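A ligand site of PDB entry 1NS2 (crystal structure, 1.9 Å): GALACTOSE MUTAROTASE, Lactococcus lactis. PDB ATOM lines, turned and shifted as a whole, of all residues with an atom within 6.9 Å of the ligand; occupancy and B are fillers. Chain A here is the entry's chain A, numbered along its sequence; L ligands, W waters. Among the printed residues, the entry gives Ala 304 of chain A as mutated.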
ATOM      1  N   ASP A  58      26.386  26.630 -12.401  1.00  0.00           N
ATOM      2  CA  ASP A  58      26.775  25.897 -13.576  1.00  0.00           C
ATOM      3  C   ASP A  58      27.857  26.715 -14.191  1.00  0.00           C
ATOM      4  O   ASP A  58      27.610  27.859 -14.524  1.00  0.00           O
ATOM      5  CB  ASP A  58      25.625  25.712 -14.565  1.00  0.00           C
ATOM      6  CG  ASP A  58      26.062  24.846 -15.698  1.00  0.00           C
ATOM      7  OD1 ASP A  58      27.191  24.454 -15.871  1.00  0.00           O
ATOM      8  OD2 ASP A  58      25.086  24.582 -16.534  1.00  0.00           O
ATOM      9  N   TYR A  60      29.555  26.148 -16.961  1.00  0.00           N
ATOM     10  CA  TYR A  60      29.749  26.062 -18.379  1.00  0.00           C
ATOM     11  C   TYR A  60      29.130  27.119 -19.242  1.00  0.00           C
ATOM     12  O   TYR A  60      29.686  27.447 -20.306  1.00  0.00           O
ATOM     13  CB  TYR A  60      29.266  24.688 -18.867  1.00  0.00           C
ATOM     14  CG  TYR A  60      30.207  23.573 -18.405  1.00  0.00           C
ATOM     15  CD1 TYR A  60      29.707  22.489 -17.688  1.00  0.00           C
ATOM     16  CD2 TYR A  60      31.569  23.578 -18.689  1.00  0.00           C
ATOM     17  CE1 TYR A  60      30.521  21.443 -17.268  1.00  0.00           C
ATOM     18  CE2 TYR A  60      32.414  22.557 -18.258  1.00  0.00           C
ATOM     19  CZ  TYR A  60      31.882  21.465 -17.556  1.00  0.00           C
ATOM     20  OH  TYR A  60      32.687  20.423 -17.139  1.00  0.00           O
ATOM     21  N   PRO A  61      27.953  27.616 -18.836  1.00  0.00           N
ATOM     22  CA  PRO A  61      27.308  28.598 -19.698  1.00  0.00           C
ATOM     23  C   PRO A  61      28.159  29.798 -20.075  1.00  0.00           C
ATOM     24  O   PRO A  61      28.688  30.470 -19.178  1.00  0.00           O
ATOM     25  CB  PRO A  61      25.970  28.964 -19.061  1.00  0.00           C
ATOM     26  CG  PRO A  61      25.773  28.030 -17.891  1.00  0.00           C
ATOM     27  CD  PRO A  61      27.086  27.279 -17.675  1.00  0.00           C
ATOM     28  N   GLY A  70      33.882  18.543 -25.165  1.00  0.00           N
ATOM     29  CA  GLY A  70      33.138  17.317 -25.359  1.00  0.00           C
ATOM     30  C   GLY A  70      33.668  16.185 -24.511  1.00  0.00           C
ATOM     31  O   GLY A  70      34.537  16.394 -23.647  1.00  0.00           O
ATOM     32  N   ARG A  71      33.127  14.988 -24.738  1.00  0.00           N
ATOM     33  CA  ARG A  71      33.550  13.851 -23.956  1.00  0.00           C
ATOM     34  C   ARG A  71      34.576  12.996 -24.641  1.00  0.00           C
ATOM     35  O   ARG A  71      34.396  12.658 -25.821  1.00  0.00           O
ATOM     36  CB  ARG A  71      32.395  12.878 -23.694  1.00  0.00           C
ATOM     37  CG  ARG A  71      31.223  13.520 -23.018  1.00  0.00           C
ATOM     38  CD  ARG A  71      30.036  12.577 -22.787  1.00  0.00           C
ATOM     39  NE  ARG A  71      29.220  13.209 -21.728  1.00  0.00           N
ATOM     40  CZ  ARG A  71      28.386  14.237 -21.896  1.00  0.00           C
ATOM     41  NH1 ARG A  71      28.110  14.782 -23.089  1.00  0.00           N
ATOM     42  NH2 ARG A  71      27.787  14.712 -20.806  1.00  0.00           N
ATOM     43  N   GLU A  90      33.753  12.624 -15.227  1.00  0.00           N
ATOM     44  CA  GLU A  90      32.381  12.266 -15.469  1.00  0.00           C
ATOM     45  C   GLU A  90      32.451  10.791 -15.652  1.00  0.00           C
ATOM     46  O   GLU A  90      32.469  10.291 -16.789  1.00  0.00           O
ATOM     47  CB  GLU A  90      31.877  12.856 -16.777  1.00  0.00           C
ATOM     48  CG  GLU A  90      30.368  12.633 -16.884  1.00  0.00           C
ATOM     49  CD  GLU A  90      29.829  12.925 -18.265  1.00  0.00           C
ATOM     50  OE1 GLU A  90      30.272  12.417 -19.264  1.00  0.00           O
ATOM     51  OE2 GLU A  90      28.836  13.773 -18.303  1.00  0.00           O
ATOM     52  N   LEU A  95      35.333  15.147 -19.547  1.00  0.00           N
ATOM     53  CA  LEU A  95      34.343  16.011 -20.201  1.00  0.00           C
ATOM     54  C   LEU A  95      34.816  17.472 -20.108  1.00  0.00           C
ATOM     55  O   LEU A  95      35.204  17.894 -19.031  1.00  0.00           O
ATOM     56  CB  LEU A  95      32.955  15.846 -19.554  1.00  0.00           C
ATOM     57  CG  LEU A  95      32.036  17.015 -19.909  1.00  0.00           C
ATOM     58  CD1 LEU A  95      31.469  16.865 -21.316  1.00  0.00           C
ATOM     59  CD2 LEU A  95      30.905  17.199 -18.900  1.00  0.00           C
ATOM     60  N   HIS A  96      34.844  18.203 -21.213  1.00  0.00           N
ATOM     61  CA  HIS A  96      35.285  19.594 -21.188  1.00  0.00           C
ATOM     62  C   HIS A  96      36.661  19.853 -20.550  1.00  0.00           C
ATOM     63  O   HIS A  96      36.867  20.852 -19.840  1.00  0.00           O
ATOM     64  CB  HIS A  96      34.206  20.459 -20.535  1.00  0.00           C
ATOM     65  CG  HIS A  96      32.927  20.425 -21.329  1.00  0.00           C
ATOM     66  ND1 HIS A  96      32.962  20.146 -22.696  1.00  0.00           N
ATOM     67  CD2 HIS A  96      31.643  20.610 -20.945  1.00  0.00           C
ATOM     68  CE1 HIS A  96      31.709  20.197 -23.135  1.00  0.00           C
ATOM     69  NE2 HIS A  96      30.889  20.454 -22.111  1.00  0.00           N
ATOM     70  N   HIS A 170      30.746  27.820 -25.207  1.00  0.00           N
ATOM     71  CA  HIS A 170      29.557  27.154 -24.675  1.00  0.00           C
ATOM     72  C   HIS A 170      28.374  28.058 -24.320  1.00  0.00           C
ATOM     73  O   HIS A 170      27.732  27.889 -23.291  1.00  0.00           O
ATOM     74  CB  HIS A 170      29.904  26.246 -23.484  1.00  0.00           C
ATOM     75  CG  HIS A 170      29.108  24.959 -23.462  1.00  0.00           C
ATOM     76  ND1 HIS A 170      27.856  24.889 -22.865  1.00  0.00           N
ATOM     77  CD2 HIS A 170      29.410  23.722 -23.991  1.00  0.00           C
ATOM     78  CE1 HIS A 170      27.434  23.634 -23.048  1.00  0.00           C
ATOM     79  NE2 HIS A 170      28.343  22.897 -23.708  1.00  0.00           N
ATOM     80  N   TYR A 172      24.650  29.571 -24.564  1.00  0.00           N
ATOM     81  CA  TYR A 172      23.310  29.020 -24.704  1.00  0.00           C
ATOM     82  C   TYR A 172      22.380  30.140 -25.157  1.00  0.00           C
ATOM     83  O   TYR A 172      22.261  31.218 -24.536  1.00  0.00           O
ATOM     84  CB  TYR A 172      22.738  28.553 -23.368  1.00  0.00           C
ATOM     85  CG  TYR A 172      23.245  27.227 -22.837  1.00  0.00           C
ATOM     86  CD1 TYR A 172      24.200  27.164 -21.833  1.00  0.00           C
ATOM     87  CD2 TYR A 172      22.657  26.032 -23.249  1.00  0.00           C
ATOM     88  CE1 TYR A 172      24.611  25.944 -21.282  1.00  0.00           C
ATOM     89  CE2 TYR A 172      23.040  24.809 -22.721  1.00  0.00           C
ATOM     90  CZ  TYR A 172      24.036  24.762 -21.746  1.00  0.00           C
ATOM     91  OH  TYR A 172      24.409  23.535 -21.227  1.00  0.00           O
ATOM     92  N   GLU A 203      26.773   8.886 -23.039  1.00  0.00           N
ATOM     93  CA  GLU A 203      26.955   9.888 -24.048  1.00  0.00           C
ATOM     94  C   GLU A 203      28.244   9.823 -24.823  1.00  0.00           C
ATOM     95  O   GLU A 203      28.589  10.775 -25.486  1.00  0.00           O
ATOM     96  CB  GLU A 203      26.628  11.325 -23.568  1.00  0.00           C
ATOM     97  CG  GLU A 203      25.125  11.595 -23.336  1.00  0.00           C
ATOM     98  CD  GLU A 203      24.719  12.554 -22.229  1.00  0.00           C
ATOM     99  OE1 GLU A 203      24.899  12.361 -21.017  1.00  0.00           O
ATOM    100  OE2 GLU A 203      24.051  13.586 -22.682  1.00  0.00           O
ATOM    101  N   VAL A 239      18.281  10.998 -25.147  1.00  0.00           N
ATOM    102  CA  VAL A 239      18.763  12.179 -24.469  1.00  0.00           C
ATOM    103  C   VAL A 239      17.669  13.153 -24.044  1.00  0.00           C
ATOM    104  O   VAL A 239      17.887  14.057 -23.236  1.00  0.00           O
ATOM    105  CB  VAL A 239      19.832  12.755 -25.424  1.00  0.00           C
ATOM    106  CG1 VAL A 239      19.645  14.152 -25.907  1.00  0.00           C
ATOM    107  CG2 VAL A 239      21.234  12.380 -24.988  1.00  0.00           C
ATOM    108  N   ILE A 242      18.199  17.125 -27.880  1.00  0.00           N
ATOM    109  CA  ILE A 242      19.325  16.967 -28.777  1.00  0.00           C
ATOM    110  C   ILE A 242      20.581  17.174 -27.950  1.00  0.00           C
ATOM    111  O   ILE A 242      20.580  18.015 -27.045  1.00  0.00           O
ATOM    112  CB  ILE A 242      19.281  17.896 -29.966  1.00  0.00           C
ATOM    113  CG1 ILE A 242      17.944  17.731 -30.681  1.00  0.00           C
ATOM    114  CG2 ILE A 242      20.438  17.612 -30.954  1.00  0.00           C
ATOM    115  CD1 ILE A 242      17.628  18.915 -31.594  1.00  0.00           C
ATOM    116  N   ASP A 243      21.604  16.389 -28.254  1.00  0.00           N
ATOM    117  CA  ASP A 243      22.891  16.474 -27.573  1.00  0.00           C
ATOM    118  C   ASP A 243      23.874  15.806 -28.497  1.00  0.00           C
ATOM    119  O   ASP A 243      24.454  14.794 -28.162  1.00  0.00           O
ATOM    120  CB  ASP A 243      22.908  15.821 -26.173  1.00  0.00           C
ATOM    121  CG  ASP A 243      24.075  16.296 -25.354  1.00  0.00           C
ATOM    122  OD1 ASP A 243      24.957  17.007 -25.790  1.00  0.00           O
ATOM    123  OD2 ASP A 243      24.016  15.950 -24.107  1.00  0.00           O
ATOM    124  N   HIS A 244      24.020  16.389 -29.703  1.00  0.00           N
ATOM    125  CA  HIS A 244      24.849  15.764 -30.692  1.00  0.00           C
ATOM    126  C   HIS A 244      25.584  16.664 -31.620  1.00  0.00           C
ATOM    127  O   HIS A 244      25.138  17.758 -31.959  1.00  0.00           O
ATOM    128  CB  HIS A 244      23.852  15.109 -31.697  1.00  0.00           C
ATOM    129  CG  HIS A 244      23.067  13.988 -31.079  1.00  0.00           C
ATOM    130  ND1 HIS A 244      21.906  14.216 -30.342  1.00  0.00           N
ATOM    131  CD2 HIS A 244      23.302  12.652 -31.150  1.00  0.00           C
ATOM    132  CE1 HIS A 244      21.465  13.048 -29.921  1.00  0.00           C
ATOM    133  NE2 HIS A 244      22.286  12.089 -30.414  1.00  0.00           N
ATOM    134  N   VAL A 277      28.075  21.168 -32.265  1.00  0.00           N
ATOM    135  CA  VAL A 277      27.462  20.339 -31.260  1.00  0.00           C
ATOM    136  C   VAL A 277      26.232  21.036 -30.671  1.00  0.00           C
ATOM    137  O   VAL A 277      26.282  22.093 -30.031  1.00  0.00           O
ATOM    138  CB  VAL A 277      28.479  19.961 -30.202  1.00  0.00           C
ATOM    139  CG1 VAL A 277      27.757  19.120 -29.141  1.00  0.00           C
ATOM    140  CG2 VAL A 277      29.584  19.153 -30.883  1.00  0.00           C
ATOM    141  N   ILE A 278      25.088  20.450 -30.908  1.00  0.00           N
ATOM    142  CA  ILE A 278      23.856  21.076 -30.439  1.00  0.00           C
ATOM    143  C   ILE A 278      23.261  20.346 -29.256  1.00  0.00           C
ATOM    144  O   ILE A 278      22.950  19.145 -29.353  1.00  0.00           O
ATOM    145  CB  ILE A 278      22.838  21.137 -31.587  1.00  0.00           C
ATOM    146  CG1 ILE A 278      23.327  22.096 -32.661  1.00  0.00           C
ATOM    147  CG2 ILE A 278      21.452  21.556 -31.101  1.00  0.00           C
ATOM    148  CD1 ILE A 278      22.501  21.987 -33.916  1.00  0.00           C
ATOM    149  N   PHE A 279      23.148  21.092 -28.144  1.00  0.00           N
ATOM    150  CA  PHE A 279      22.619  20.573 -26.898  1.00  0.00           C
ATOM    151  C   PHE A 279      21.499  21.496 -26.469  1.00  0.00           C
ATOM    152  O   PHE A 279      21.734  22.704 -26.379  1.00  0.00           O
ATOM    153  CB  PHE A 279      23.752  20.510 -25.838  1.00  0.00           C
ATOM    154  CG  PHE A 279      23.327  20.220 -24.418  1.00  0.00           C
ATOM    155  CD1 PHE A 279      22.671  19.035 -24.103  1.00  0.00           C
ATOM    156  CD2 PHE A 279      23.569  21.174 -23.419  1.00  0.00           C
ATOM    157  CE1 PHE A 279      22.307  18.747 -22.779  1.00  0.00           C
ATOM    158  CE2 PHE A 279      23.192  20.924 -22.106  1.00  0.00           C
ATOM    159  CZ  PHE A 279      22.581  19.707 -21.796  1.00  0.00           C
ATOM    160  N   ASN A 282      18.735  19.819 -21.834  1.00  0.00           N
ATOM    161  CA  ASN A 282      17.905  18.664 -21.453  1.00  0.00           C
ATOM    162  C   ASN A 282      18.055  18.356 -19.963  1.00  0.00           C
ATOM    163  O   ASN A 282      18.395  17.221 -19.615  1.00  0.00           O
ATOM    164  CB  ASN A 282      18.426  17.445 -22.264  1.00  0.00           C
ATOM    165  CG  ASN A 282      18.470  17.699 -23.779  1.00  0.00           C
ATOM    166  OD1 ASN A 282      17.676  18.488 -24.304  1.00  0.00           O
ATOM    167  ND2 ASN A 282      19.388  17.032 -24.496  1.00  0.00           N
ATOM    168  N   PHE A 283      17.830  19.365 -19.088  1.00  0.00           N
ATOM    169  CA  PHE A 283      18.018  19.225 -17.639  1.00  0.00           C
ATOM    170  C   PHE A 283      16.831  18.764 -16.814  1.00  0.00           C
ATOM    171  O   PHE A 283      16.825  18.821 -15.564  1.00  0.00           O
ATOM    172  CB  PHE A 283      18.653  20.462 -16.983  1.00  0.00           C
ATOM    173  CG  PHE A 283      19.945  20.971 -17.617  1.00  0.00           C
ATOM    174  CD1 PHE A 283      19.962  22.158 -18.351  1.00  0.00           C
ATOM    175  CD2 PHE A 283      21.157  20.301 -17.431  1.00  0.00           C
ATOM    176  CE1 PHE A 283      21.148  22.664 -18.894  1.00  0.00           C
ATOM    177  CE2 PHE A 283      22.352  20.779 -17.973  1.00  0.00           C
ATOM    178  CZ  PHE A 283      22.337  21.965 -18.716  1.00  0.00           C
ATOM    179  N   THR A 302      22.669  25.214 -27.514  1.00  0.00           N
ATOM    180  CA  THR A 302      23.983  25.628 -27.890  1.00  0.00           C
ATOM    181  C   THR A 302      24.265  25.415 -29.331  1.00  0.00           C
ATOM    182  O   THR A 302      23.621  24.583 -29.971  1.00  0.00           O
ATOM    183  CB  THR A 302      25.030  24.719 -27.227  1.00  0.00           C
ATOM    184  OG1 THR A 302      24.869  23.373 -27.694  1.00  0.00           O
ATOM    185  CG2 THR A 302      25.085  24.788 -25.716  1.00  0.00           C
ATOM    186  N   ALA A 304      27.927  24.750 -30.302  1.00  0.00           N
ATOM    187  CA  ALA A 304      29.355  24.669 -30.026  1.00  0.00           C
ATOM    188  C   ALA A 304      30.116  24.275 -31.254  1.00  0.00           C
ATOM    189  O   ALA A 304      30.080  23.108 -31.666  1.00  0.00           O
ATOM    190  CB  ALA A 304      29.679  23.687 -28.899  1.00  0.00           C
HETATM  191  C1  LIG L   1      27.787  19.730 -23.437  1.00  0.00           C
HETATM  192  C2  LIG L   1      27.301  18.270 -23.400  1.00  0.00           C
HETATM  193  C3  LIG L   1      26.030  18.090 -22.583  1.00  0.00           C
HETATM  194  C4  LIG L   1      26.297  18.622 -21.196  1.00  0.00           C
HETATM  195  C5  LIG L   1      26.760  20.084 -21.263  1.00  0.00           C
HETATM  196  C6  LIG L   1      27.220  20.548 -19.884  1.00  0.00           C
HETATM  197  O1  LIG L   1      26.974  20.598 -24.216  1.00  0.00           O
HETATM  198  O2  LIG L   1      27.015  17.708 -24.681  1.00  0.00           O
HETATM  199  O3  LIG L   1      25.775  16.676 -22.478  1.00  0.00           O
HETATM  200  O4  LIG L   1      27.310  17.817 -20.557  1.00  0.00           O
HETATM  201  O5  LIG L   1      27.924  20.284 -22.113  1.00  0.00           O
HETATM  202  O6  LIG L   1      26.370  21.596 -19.574  1.00  0.00           O
HETATM  203  O   HOH W   1      29.756  17.695 -26.106  1.00  0.00           O
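Residues that only touch the ligand: Phe 279, Glu 203 and Tyr 60.
Hydrophobic or aromatic side chains within 4 Å of the ligand: Tyr 60, His 96, His 170 and Phe 279.
Within 4 Å of the ligand: Tyr 60, Arg 71, His 96, His 170, Tyr 172, Glu 203, Asp 243 and Phe 279.
The nearest printed residue that does not touch the ligand is Leu 95 (4.01 Å).
OH of Tyr 172 sits at hydrogen-bond distance from O6 of the ligand (3.2 Å).
O5 of the ligand lies within hydrogen-bond range of NE2 of His 96 (3.0 Å).
An oxygen (O1) of the ligand lies within hydrogen-bond range of a ring nitrogen (NE2) of His 170, at 2.7 Å.
The guanidinium group of Arg 71 sits at hydrogen-bond distance from an oxygen (O3) of the ligand (3.1 Å).
The side-chain carboxylate of Asp 243 lies within hydrogen-bond range of an oxygen (O2) of the ligand.
The backbone NH of Tyr 60 sits at hydrogen-bond distance from the side-chain carboxylate of Asp 58 (3.1 Å).
The backbone NH (N) of His 96 is in hydrogen-bond range of the backbone carbonyl oxygen (O) of Gly 70 (3.0 Å).
The backbone NH (N) of Asp 243 sits close to the backbone carbonyl oxygen (O) of Ile 278 (3.3 Å).
The guanidinium group (NH2) of Arg 71 is in salt-bridge range of the side-chain carboxylate (OE1) of Glu 203 (3.7 Å).
The backbone NH (N) of Phe 279 lies within hydrogen-bond range of the side-chain hydroxyl (OG1) of Thr 302 (2.9 Å).
The guanidinium group of Arg 71 lies within salt-bridge range of the side-chain carboxylate of Glu 90 (2.8 Å).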
